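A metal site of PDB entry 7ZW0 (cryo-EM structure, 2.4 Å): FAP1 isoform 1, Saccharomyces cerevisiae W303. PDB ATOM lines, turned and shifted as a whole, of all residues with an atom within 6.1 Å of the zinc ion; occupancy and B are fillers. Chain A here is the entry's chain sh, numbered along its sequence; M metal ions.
O of Glu 378 lies close to SG of Cys 380 (3.3 Å). The backbone carbonyl oxygen (O) of His 365 lies within hydrogen-bond range of the backbone NH (N) of Leu 360, 3.4 Å away. The side-chain sulfur (SG) of Cys 362 lies close to the backbone NH (N) of Lys 364, 3.6 Å away.
CG of Leu 360 touches the zinc ion, 3.4 Å away. CB of Cys 399 touches the zinc ion, at 3.0 Å. Within 4 Å of the zinc ion: Leu 360, Cys 362, His 365, Cys 380 and Cys 399. The nearest printed residue that does not touch the zinc ion is Glu 378 (4.7 Å).
The zinc ion is bound by SG of Cys 380 (2.3 Å), NE2 of His 365 (2.4 Å) and SG of Cys 362 (2.7 Å).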
ATOM      1  N   LEU A 360      16.928 -22.782 -26.382  1.00  0.00           N
ATOM      2  CA  LEU A 360      17.059 -22.300 -25.010  1.00  0.00           C
ATOM      3  C   LEU A 360      17.383 -23.440 -24.073  1.00  0.00           C
ATOM      4  O   LEU A 360      17.147 -24.608 -24.402  1.00  0.00           O
ATOM      5  CB  LEU A 360      15.791 -21.574 -24.559  1.00  0.00           C
ATOM      6  CG  LEU A 360      15.883 -20.048 -24.574  1.00  0.00           C
ATOM      7  CD1 LEU A 360      17.094 -19.600 -23.771  1.00  0.00           C
ATOM      8  CD2 LEU A 360      15.917 -19.494 -25.985  1.00  0.00           C
ATOM      9  N   LYS A 361      17.932 -23.129 -22.899  1.00  0.00           N
ATOM     10  CA  LYS A 361      18.210 -24.168 -21.924  1.00  0.00           C
ATOM     11  C   LYS A 361      16.912 -24.831 -21.524  1.00  0.00           C
ATOM     12  O   LYS A 361      16.844 -26.056 -21.392  1.00  0.00           O
ATOM     13  CB  LYS A 361      18.896 -23.572 -20.691  1.00  0.00           C
ATOM     14  CG  LYS A 361      19.771 -24.559 -19.936  1.00  0.00           C
ATOM     15  CD  LYS A 361      21.023 -24.905 -20.744  1.00  0.00           C
ATOM     16  CE  LYS A 361      21.878 -25.939 -20.037  1.00  0.00           C
ATOM     17  NZ  LYS A 361      21.164 -27.233 -19.867  1.00  0.00           N
ATOM     18  N   CYS A 362      15.861 -24.032 -21.327  1.00  0.00           N
ATOM     19  CA  CYS A 362      14.555 -24.593 -21.023  1.00  0.00           C
ATOM     20  C   CYS A 362      14.054 -25.423 -22.193  1.00  0.00           C
ATOM     21  O   CYS A 362      13.466 -26.489 -21.998  1.00  0.00           O
ATOM     22  CB  CYS A 362      13.553 -23.479 -20.689  1.00  0.00           C
ATOM     23  SG  CYS A 362      13.287 -22.281 -22.014  1.00  0.00           S
ATOM     24  N   GLY A 363      14.280 -24.941 -23.412  1.00  0.00           N
ATOM     25  CA  GLY A 363      13.854 -25.668 -24.596  1.00  0.00           C
ATOM     26  C   GLY A 363      12.421 -25.424 -24.998  1.00  0.00           C
ATOM     27  O   GLY A 363      11.929 -26.022 -25.943  1.00  0.00           O
ATOM     28  N   LYS A 364      11.735 -24.544 -24.275  1.00  0.00           N
ATOM     29  CA  LYS A 364      10.363 -24.210 -24.615  1.00  0.00           C
ATOM     30  C   LYS A 364      10.319 -23.539 -25.980  1.00  0.00           C
ATOM     31  O   LYS A 364       9.433 -23.811 -26.779  1.00  0.00           O
ATOM     32  CB  LYS A 364       9.746 -23.269 -23.560  1.00  0.00           C
ATOM     33  CG  LYS A 364       9.070 -23.971 -22.396  1.00  0.00           C
ATOM     34  CD  LYS A 364      10.072 -24.638 -21.474  1.00  0.00           C
ATOM     35  CE  LYS A 364       9.395 -25.300 -20.279  1.00  0.00           C
ATOM     36  NZ  LYS A 364      10.387 -25.943 -19.375  1.00  0.00           N
ATOM     37  N   HIS A 365      11.295 -22.675 -26.238  1.00  0.00           N
ATOM     38  CA  HIS A 365      11.347 -22.011 -27.522  1.00  0.00           C
ATOM     39  C   HIS A 365      12.767 -21.930 -28.026  1.00  0.00           C
ATOM     40  O   HIS A 365      13.706 -22.169 -27.265  1.00  0.00           O
ATOM     41  CB  HIS A 365      10.758 -20.603 -27.418  1.00  0.00           C
ATOM     42  CG  HIS A 365      11.082 -19.899 -26.140  1.00  0.00           C
ATOM     43  ND1 HIS A 365      10.119 -19.456 -25.269  1.00  0.00           N
ATOM     44  CD2 HIS A 365      12.276 -19.581 -25.570  1.00  0.00           C
ATOM     45  CE1 HIS A 365      10.693 -18.874 -24.224  1.00  0.00           C
ATOM     46  NE2 HIS A 365      12.009 -18.943 -24.386  1.00  0.00           N
ATOM     47  N   GLU A 378      20.472 -17.801 -20.935  1.00  0.00           N
ATOM     48  CA  GLU A 378      19.393 -18.577 -20.335  1.00  0.00           C
ATOM     49  C   GLU A 378      18.198 -17.741 -19.875  1.00  0.00           C
ATOM     50  O   GLU A 378      17.057 -18.140 -20.087  1.00  0.00           O
ATOM     51  CB  GLU A 378      19.922 -19.473 -19.202  1.00  0.00           C
ATOM     52  CG  GLU A 378      21.019 -20.421 -19.652  1.00  0.00           C
ATOM     53  CD  GLU A 378      21.473 -21.360 -18.551  1.00  0.00           C
ATOM     54  OE1 GLU A 378      22.447 -22.107 -18.766  1.00  0.00           O
ATOM     55  OE2 GLU A 378      20.848 -21.342 -17.468  1.00  0.00           O
ATOM     56  N   PRO A 379      18.433 -16.573 -19.233  1.00  0.00           N
ATOM     57  CA  PRO A 379      17.263 -15.745 -18.932  1.00  0.00           C
ATOM     58  C   PRO A 379      16.649 -15.265 -20.235  1.00  0.00           C
ATOM     59  O   PRO A 379      17.383 -14.937 -21.160  1.00  0.00           O
ATOM     60  CB  PRO A 379      17.835 -14.568 -18.139  1.00  0.00           C
ATOM     61  CG  PRO A 379      19.320 -14.691 -18.208  1.00  0.00           C
ATOM     62  CD  PRO A 379      19.600 -16.144 -18.439  1.00  0.00           C
ATOM     63  N   CYS A 380      15.325 -15.213 -20.303  1.00  0.00           N
ATOM     64  CA  CYS A 380      14.685 -14.848 -21.566  1.00  0.00           C
ATOM     65  C   CYS A 380      13.956 -13.521 -21.516  1.00  0.00           C
ATOM     66  O   CYS A 380      13.135 -13.298 -20.627  1.00  0.00           O
ATOM     67  CB  CYS A 380      13.695 -15.944 -21.962  1.00  0.00           C
ATOM     68  SG  CYS A 380      14.379 -17.615 -21.967  1.00  0.00           S
ATOM     69  N   GLN A 382      11.954 -12.854 -23.641  1.00  0.00           N
ATOM     70  CA  GLN A 382      10.641 -13.414 -23.940  1.00  0.00           C
ATOM     71  C   GLN A 382       9.963 -13.970 -22.694  1.00  0.00           C
ATOM     72  O   GLN A 382      10.450 -14.928 -22.080  1.00  0.00           O
ATOM     73  CB  GLN A 382      10.747 -14.485 -25.021  1.00  0.00           C
ATOM     74  CG  GLN A 382      12.088 -15.216 -25.045  1.00  0.00           C
ATOM     75  CD  GLN A 382      12.249 -16.102 -26.271  1.00  0.00           C
ATOM     76  OE1 GLN A 382      11.264 -16.510 -26.883  1.00  0.00           O
ATOM     77  NE2 GLN A 382      13.492 -16.400 -26.618  1.00  0.00           N
ATOM     78  N   PRO A 398       9.483 -14.527 -17.297  1.00  0.00           N
ATOM     79  CA  PRO A 398      10.430 -15.178 -18.206  1.00  0.00           C
ATOM     80  C   PRO A 398      10.709 -16.633 -17.856  1.00  0.00           C
ATOM     81  O   PRO A 398      10.548 -17.030 -16.700  1.00  0.00           O
ATOM     82  CB  PRO A 398      11.720 -14.358 -18.021  1.00  0.00           C
ATOM     83  CG  PRO A 398      11.593 -13.755 -16.663  1.00  0.00           C
ATOM     84  CD  PRO A 398      10.142 -13.424 -16.554  1.00  0.00           C
ATOM     85  N   CYS A 399      11.137 -17.425 -18.825  1.00  0.00           N
ATOM     86  CA  CYS A 399      11.471 -18.811 -18.542  1.00  0.00           C
ATOM     87  C   CYS A 399      12.647 -18.863 -17.581  1.00  0.00           C
ATOM     88  O   CYS A 399      13.604 -18.093 -17.715  1.00  0.00           O
ATOM     89  CB  CYS A 399      11.799 -19.563 -19.832  1.00  0.00           C
ATOM     90  SG  CYS A 399      10.383 -19.774 -20.931  1.00  0.00           S
ATOM     91  N   GLY A 400      12.588 -19.762 -16.601  1.00  0.00           N
ATOM     92  CA  GLY A 400      13.640 -19.845 -15.607  1.00  0.00           C
ATOM     93  C   GLY A 400      13.253 -19.080 -14.364  1.00  0.00           C
ATOM     94  O   GLY A 400      14.035 -18.991 -13.411  1.00  0.00           O
HETATM   95 ZN    ZN M   1      13.243 -19.613 -22.417  1.00  0.00          ZN
